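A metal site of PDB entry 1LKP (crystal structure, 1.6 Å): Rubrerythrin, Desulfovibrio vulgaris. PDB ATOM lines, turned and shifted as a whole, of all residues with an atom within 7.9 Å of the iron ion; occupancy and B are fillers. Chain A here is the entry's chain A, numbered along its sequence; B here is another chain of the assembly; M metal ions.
The iron ion is bound by SG of Cys 161 (2.3 Å), SG of Cys 174 (2.3 Å), SG of Cys 177 (2.3 Å) and SG of Cys 158 (2.3 Å).
Within 4 Å of the iron ion: Cys 158, Cys 161, Cys 174 and Cys 177. Along chain A the residues within 4 Å of the iron ion span positions 158 to 177.
SG of Cys 161 lies close to N of Tyr 163, 3.5 Å away. A ring nitrogen (NE2) of His 56 of chain B sits at hydrogen-bond distance from the backbone carbonyl oxygen (O) of Cys 161 (2.8 Å). The side-chain sulfur of Cys 174 lies close to the backbone NH of Ala 176, 3.5 Å away. N of Cys 174 sits at hydrogen-bond distance from O of His 179, 2.8 Å away. The side-chain sulfur (SG) of Cys 177 sits close to the side-chain amide oxygen (OD1) of Asn 160, at 3.3 Å. O of Cys 177 is in hydrogen-bond range of ND1 of His 179 (3.0 Å). N of Cys 158 is in hydrogen-bond range of O of Tyr 163 (2.8 Å). SG of Cys 158 lies close to N of Asn 160 (3.5 Å).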
ATOM      1  N   ARG A 157       7.342  23.220   0.762  1.00  0.00           N
ATOM      2  CA  ARG A 157       7.848  23.203  -0.611  1.00  0.00           C
ATOM      3  C   ARG A 157       7.154  24.258  -1.459  1.00  0.00           C
ATOM      4  O   ARG A 157       5.943  24.450  -1.374  1.00  0.00           O
ATOM      5  CB  ARG A 157       7.623  21.827  -1.251  1.00  0.00           C
ATOM      6  CG  ARG A 157       8.314  21.675  -2.614  1.00  0.00           C
ATOM      7  CD  ARG A 157       7.949  20.357  -3.308  1.00  0.00           C
ATOM      8  NE  ARG A 157       6.565  20.352  -3.800  1.00  0.00           N
ATOM      9  CZ  ARG A 157       6.227  20.135  -5.066  1.00  0.00           C
ATOM     10  NH1 ARG A 157       7.162  19.911  -5.978  1.00  0.00           N
ATOM     11  NH2 ARG A 157       4.945  20.139  -5.419  1.00  0.00           N
ATOM     12  N   CYS A 158       7.937  24.963  -2.276  1.00  0.00           N
ATOM     13  CA  CYS A 158       7.386  25.979  -3.161  1.00  0.00           C
ATOM     14  C   CYS A 158       6.885  25.227  -4.398  1.00  0.00           C
ATOM     15  O   CYS A 158       7.676  24.597  -5.104  1.00  0.00           O
ATOM     16  CB  CYS A 158       8.464  26.982  -3.573  1.00  0.00           C
ATOM     17  SG  CYS A 158       7.924  28.145  -4.842  1.00  0.00           S
ATOM     18  N   ARG A 159       5.589  25.286  -4.657  1.00  0.00           N
ATOM     19  CA  ARG A 159       5.050  24.588  -5.827  1.00  0.00           C
ATOM     20  C   ARG A 159       5.559  25.174  -7.141  1.00  0.00           C
ATOM     21  O   ARG A 159       5.627  24.480  -8.152  1.00  0.00           O
ATOM     22  CB  ARG A 159       3.507  24.616  -5.798  1.00  0.00           C
ATOM     23  CG  ARG A 159       2.894  23.715  -4.727  1.00  0.00           C
ATOM     24  CD  ARG A 159       1.360  23.720  -4.790  1.00  0.00           C
ATOM     25  NE  ARG A 159       0.858  23.166  -6.049  1.00  0.00           N
ATOM     26  CZ  ARG A 159       0.903  21.876  -6.384  1.00  0.00           C
ATOM     27  NH1 ARG A 159       1.419  20.971  -5.552  1.00  0.00           N
ATOM     28  NH2 ARG A 159       0.429  21.486  -7.564  1.00  0.00           N
ATOM     29  N   ASN A 160       5.937  26.447  -7.130  1.00  0.00           N
ATOM     30  CA  ASN A 160       6.419  27.099  -8.352  1.00  0.00           C
ATOM     31  C   ASN A 160       7.815  26.651  -8.807  1.00  0.00           C
ATOM     32  O   ASN A 160       8.028  26.436 -10.014  1.00  0.00           O
ATOM     33  CB  ASN A 160       6.427  28.619  -8.193  1.00  0.00           C
ATOM     34  CG  ASN A 160       6.712  29.348  -9.493  1.00  0.00           C
ATOM     35  OD1 ASN A 160       7.735  30.032  -9.634  1.00  0.00           O
ATOM     36  ND2 ASN A 160       5.807  29.202 -10.457  1.00  0.00           N
ATOM     37  N   CYS A 161       8.739  26.493  -7.873  1.00  0.00           N
ATOM     38  CA  CYS A 161      10.109  26.111  -8.236  1.00  0.00           C
ATOM     39  C   CYS A 161      10.724  24.939  -7.480  1.00  0.00           C
ATOM     40  O   CYS A 161      11.832  24.514  -7.794  1.00  0.00           O
ATOM     41  CB  CYS A 161      11.040  27.315  -8.087  1.00  0.00           C
ATOM     42  SG  CYS A 161      11.465  27.701  -6.362  1.00  0.00           S
ATOM     43  N   GLY A 162      10.014  24.419  -6.484  1.00  0.00           N
ATOM     44  CA  GLY A 162      10.548  23.285  -5.749  1.00  0.00           C
ATOM     45  C   GLY A 162      11.435  23.596  -4.550  1.00  0.00           C
ATOM     46  O   GLY A 162      11.943  22.682  -3.911  1.00  0.00           O
ATOM     47  N   TYR A 163      11.652  24.870  -4.257  1.00  0.00           N
ATOM     48  CA  TYR A 163      12.481  25.235  -3.111  1.00  0.00           C
ATOM     49  C   TYR A 163      11.877  24.629  -1.841  1.00  0.00           C
ATOM     50  O   TYR A 163      10.661  24.577  -1.686  1.00  0.00           O
ATOM     51  CB  TYR A 163      12.560  26.752  -2.958  1.00  0.00           C
ATOM     52  CG  TYR A 163      13.358  27.186  -1.751  1.00  0.00           C
ATOM     53  CD1 TYR A 163      14.743  27.094  -1.740  1.00  0.00           C
ATOM     54  CD2 TYR A 163      12.713  27.639  -0.598  1.00  0.00           C
ATOM     55  CE1 TYR A 163      15.481  27.446  -0.602  1.00  0.00           C
ATOM     56  CE2 TYR A 163      13.434  27.974   0.548  1.00  0.00           C
ATOM     57  CZ  TYR A 163      14.816  27.882   0.537  1.00  0.00           C
ATOM     58  OH  TYR A 163      15.541  28.231   1.654  1.00  0.00           O
ATOM     59  N   VAL A 164      12.737  24.180  -0.935  1.00  0.00           N
ATOM     60  CA  VAL A 164      12.278  23.604   0.316  1.00  0.00           C
ATOM     61  C   VAL A 164      12.711  24.507   1.457  1.00  0.00           C
ATOM     62  O   VAL A 164      13.905  24.824   1.606  1.00  0.00           O
ATOM     63  CB  VAL A 164      12.875  22.196   0.533  1.00  0.00           C
ATOM     64  CG1 VAL A 164      12.419  21.641   1.883  1.00  0.00           C
ATOM     65  CG2 VAL A 164      12.427  21.273  -0.591  1.00  0.00           C
ATOM     66  N   LEU A 173       8.189  35.279   0.832  1.00  0.00           N
ATOM     67  CA  LEU A 173       8.649  35.210  -0.555  1.00  0.00           C
ATOM     68  C   LEU A 173       9.626  34.050  -0.690  1.00  0.00           C
ATOM     69  O   LEU A 173      10.459  33.832   0.192  1.00  0.00           O
ATOM     70  CB  LEU A 173       9.360  36.502  -0.956  1.00  0.00           C
ATOM     71  CG  LEU A 173       8.502  37.758  -1.150  1.00  0.00           C
ATOM     72  CD1 LEU A 173       9.409  38.935  -1.512  1.00  0.00           C
ATOM     73  CD2 LEU A 173       7.475  37.527  -2.260  1.00  0.00           C
ATOM     74  N   CYS A 174       9.516  33.301  -1.777  1.00  0.00           N
ATOM     75  CA  CYS A 174      10.412  32.177  -2.001  1.00  0.00           C
ATOM     76  C   CYS A 174      11.807  32.741  -2.301  1.00  0.00           C
ATOM     77  O   CYS A 174      11.978  33.575  -3.181  1.00  0.00           O
ATOM     78  CB  CYS A 174       9.931  31.338  -3.192  1.00  0.00           C
ATOM     79  SG  CYS A 174      11.042  29.967  -3.587  1.00  0.00           S
ATOM     80  N   PRO A 175      12.826  32.298  -1.550  1.00  0.00           N
ATOM     81  CA  PRO A 175      14.173  32.815  -1.804  1.00  0.00           C
ATOM     82  C   PRO A 175      14.771  32.414  -3.147  1.00  0.00           C
ATOM     83  O   PRO A 175      15.746  33.021  -3.603  1.00  0.00           O
ATOM     84  CB  PRO A 175      14.976  32.286  -0.619  1.00  0.00           C
ATOM     85  CG  PRO A 175      14.292  30.988  -0.317  1.00  0.00           C
ATOM     86  CD  PRO A 175      12.822  31.358  -0.418  1.00  0.00           C
ATOM     87  N   ALA A 176      14.197  31.397  -3.782  1.00  0.00           N
ATOM     88  CA  ALA A 176      14.686  30.945  -5.080  1.00  0.00           C
ATOM     89  C   ALA A 176      13.994  31.635  -6.260  1.00  0.00           C
ATOM     90  O   ALA A 176      14.654  32.282  -7.065  1.00  0.00           O
ATOM     91  CB  ALA A 176      14.511  29.428  -5.201  1.00  0.00           C
ATOM     92  N   CYS A 177      12.678  31.523  -6.346  1.00  0.00           N
ATOM     93  CA  CYS A 177      11.939  32.112  -7.461  1.00  0.00           C
ATOM     94  C   CYS A 177      11.226  33.436  -7.186  1.00  0.00           C
ATOM     95  O   CYS A 177      10.595  34.001  -8.090  1.00  0.00           O
ATOM     96  CB  CYS A 177      10.929  31.100  -8.009  1.00  0.00           C
ATOM     97  SG  CYS A 177       9.496  30.845  -6.935  1.00  0.00           S
ATOM     98  N   ALA A 178      11.305  33.918  -5.956  1.00  0.00           N
ATOM     99  CA  ALA A 178      10.679  35.185  -5.570  1.00  0.00           C
ATOM    100  C   ALA A 178       9.160  35.233  -5.627  1.00  0.00           C
ATOM    101  O   ALA A 178       8.572  36.313  -5.569  1.00  0.00           O
ATOM    102  CB  ALA A 178      11.272  36.327  -6.404  1.00  0.00           C
ATOM    103  N   HIS A 179       8.509  34.079  -5.770  1.00  0.00           N
ATOM    104  CA  HIS A 179       7.054  34.073  -5.798  1.00  0.00           C
ATOM    105  C   HIS A 179       6.531  34.143  -4.353  1.00  0.00           C
ATOM    106  O   HIS A 179       7.239  33.781  -3.419  1.00  0.00           O
ATOM    107  CB  HIS A 179       6.527  32.848  -6.527  1.00  0.00           C
ATOM    108  CG  HIS A 179       6.595  32.976  -8.018  1.00  0.00           C
ATOM    109  ND1 HIS A 179       7.749  33.320  -8.688  1.00  0.00           N
ATOM    110  CD2 HIS A 179       5.640  32.840  -8.965  1.00  0.00           C
ATOM    111  CE1 HIS A 179       7.499  33.386  -9.980  1.00  0.00           C
ATOM    112  NE2 HIS A 179       6.230  33.111 -10.182  1.00  0.00           N
ATOM    113  N   PRO A 180       5.293  34.628  -4.163  1.00  0.00           N
ATOM    114  CA  PRO A 180       4.716  34.746  -2.829  1.00  0.00           C
ATOM    115  C   PRO A 180       4.396  33.462  -2.074  1.00  0.00           C
ATOM    116  O   PRO A 180       4.301  32.377  -2.656  1.00  0.00           O
ATOM    117  CB  PRO A 180       3.480  35.606  -3.063  1.00  0.00           C
ATOM    118  CG  PRO A 180       3.060  35.211  -4.436  1.00  0.00           C
ATOM    119  CD  PRO A 180       4.364  35.141  -5.192  1.00  0.00           C
ATOM    120  N   HIS A 183       2.382  30.122  -2.916  1.00  0.00           N
ATOM    121  CA  HIS A 183       2.832  28.934  -3.641  1.00  0.00           C
ATOM    122  C   HIS A 183       3.319  27.777  -2.772  1.00  0.00           C
ATOM    123  O   HIS A 183       3.574  26.683  -3.278  1.00  0.00           O
ATOM    124  CB  HIS A 183       3.919  29.324  -4.634  1.00  0.00           C
ATOM    125  CG  HIS A 183       3.424  30.199  -5.753  1.00  0.00           C
ATOM    126  ND1 HIS A 183       3.025  29.688  -6.970  1.00  0.00           N
ATOM    127  CD2 HIS A 183       3.202  31.526  -5.809  1.00  0.00           C
ATOM    128  CE1 HIS A 183       2.580  30.673  -7.725  1.00  0.00           C
ATOM    129  NE2 HIS A 183       2.674  31.801  -7.046  1.00  0.00           N
ATOM    130  N   PHE A 184       3.447  28.005  -1.466  1.00  0.00           N
ATOM    131  CA  PHE A 184       3.951  26.955  -0.585  1.00  0.00           C
ATOM    132  C   PHE A 184       2.933  25.946  -0.056  1.00  0.00           C
ATOM    133  O   PHE A 184       1.752  26.248   0.129  1.00  0.00           O
ATOM    134  CB  PHE A 184       4.708  27.568   0.588  1.00  0.00           C
ATOM    135  CG  PHE A 184       6.065  28.106   0.219  1.00  0.00           C
ATOM    136  CD1 PHE A 184       6.202  29.381  -0.332  1.00  0.00           C
ATOM    137  CD2 PHE A 184       7.208  27.322   0.395  1.00  0.00           C
ATOM    138  CE1 PHE A 184       7.453  29.863  -0.715  1.00  0.00           C
ATOM    139  CE2 PHE A 184       8.469  27.796   0.007  1.00  0.00           C
ATOM    140  CZ  PHE A 184       8.587  29.068  -0.541  1.00  0.00           C
ATOM    141  N   GLN B  52       9.268  23.509 -13.022  1.00  0.00           N
ATOM    142  CA  GLN B  52      10.022  24.199 -11.991  1.00  0.00           C
ATOM    143  C   GLN B  52      11.373  24.656 -12.542  1.00  0.00           C
ATOM    144  O   GLN B  52      11.862  25.715 -12.149  1.00  0.00           O
ATOM    145  CB  GLN B  52      10.159  23.310 -10.756  1.00  0.00           C
ATOM    146  CG  GLN B  52       8.785  22.977 -10.167  1.00  0.00           C
ATOM    147  CD  GLN B  52       8.813  22.181  -8.887  1.00  0.00           C
ATOM    148  OE1 GLN B  52       9.722  21.395  -8.648  1.00  0.00           O
ATOM    149  NE2 GLN B  52       7.782  22.357  -8.054  1.00  0.00           N
ATOM    150  N   GLU B  55      10.983  27.839 -14.107  1.00  0.00           N
ATOM    151  CA  GLU B  55      10.953  28.932 -13.136  1.00  0.00           C
ATOM    152  C   GLU B  55      12.355  29.310 -12.636  1.00  0.00           C
ATOM    153  O   GLU B  55      12.619  30.468 -12.350  1.00  0.00           O
ATOM    154  CB  GLU B  55      10.015  28.590 -11.987  1.00  0.00           C
ATOM    155  CG  GLU B  55       8.555  28.444 -12.447  1.00  0.00           C
ATOM    156  CD  GLU B  55       8.014  29.706 -13.100  1.00  0.00           C
ATOM    157  OE1 GLU B  55       8.214  30.810 -12.544  1.00  0.00           O
ATOM    158  OE2 GLU B  55       7.361  29.608 -14.176  1.00  0.00           O
ATOM    159  N   HIS B  56      13.245  28.329 -12.504  1.00  0.00           N
ATOM    160  CA  HIS B  56      14.612  28.646 -12.092  1.00  0.00           C
ATOM    161  C   HIS B  56      15.203  29.502 -13.212  1.00  0.00           C
ATOM    162  O   HIS B  56      15.850  30.517 -12.963  1.00  0.00           O
ATOM    163  CB  HIS B  56      15.470  27.379 -11.969  1.00  0.00           C
ATOM    164  CG  HIS B  56      15.037  26.446 -10.896  1.00  0.00           C
ATOM    165  ND1 HIS B  56      15.538  25.166 -10.779  1.00  0.00           N
ATOM    166  CD2 HIS B  56      14.128  26.585  -9.894  1.00  0.00           C
ATOM    167  CE1 HIS B  56      14.958  24.554  -9.752  1.00  0.00           C
ATOM    168  NE2 HIS B  56      14.102  25.397  -9.205  1.00  0.00           N
ATOM    169  N   ARG B  59      13.935  33.169 -13.256  1.00  0.00           N
ATOM    170  CA  ARG B  59      14.544  34.006 -12.228  1.00  0.00           C
ATOM    171  C   ARG B  59      15.932  34.438 -12.697  1.00  0.00           C
ATOM    172  O   ARG B  59      16.302  35.604 -12.577  1.00  0.00           O
ATOM    173  CB  ARG B  59      14.668  33.238 -10.901  1.00  0.00           C
ATOM    174  CG  ARG B  59      15.214  34.086  -9.743  1.00  0.00           C
ATOM    175  CD  ARG B  59      14.206  35.148  -9.309  1.00  0.00           C
ATOM    176  NE  ARG B  59      14.785  36.224  -8.514  1.00  0.00           N
ATOM    177  CZ  ARG B  59      14.993  36.188  -7.199  1.00  0.00           C
ATOM    178  NH1 ARG B  59      14.676  35.115  -6.495  1.00  0.00           N
ATOM    179  NH2 ARG B  59      15.506  37.245  -6.588  1.00  0.00           N
ATOM    180  N   SER B 123      19.767  28.998  -3.219  1.00  0.00           N
ATOM    181  CA  SER B 123      18.383  28.596  -3.028  1.00  0.00           C
ATOM    182  C   SER B 123      17.929  27.619  -4.109  1.00  0.00           C
ATOM    183  O   SER B 123      17.234  26.653  -3.832  1.00  0.00           O
ATOM    184  CB  SER B 123      17.480  29.828  -3.011  1.00  0.00           C
ATOM    185  OG  SER B 123      17.791  30.640  -1.884  1.00  0.00           O
ATOM    186  N   ALA B 127      16.406  23.373  -4.214  1.00  0.00           N
ATOM    187  CA  ALA B 127      15.333  22.789  -5.025  1.00  0.00           C
ATOM    188  C   ALA B 127      15.850  21.583  -5.796  1.00  0.00           C
ATOM    189  O   ALA B 127      15.186  20.542  -5.852  1.00  0.00           O
ATOM    190  CB  ALA B 127      14.795  23.828  -6.004  1.00  0.00           C
HETATM  191 FE    FE M   1       9.970  29.116  -5.437  1.00  0.00          FE
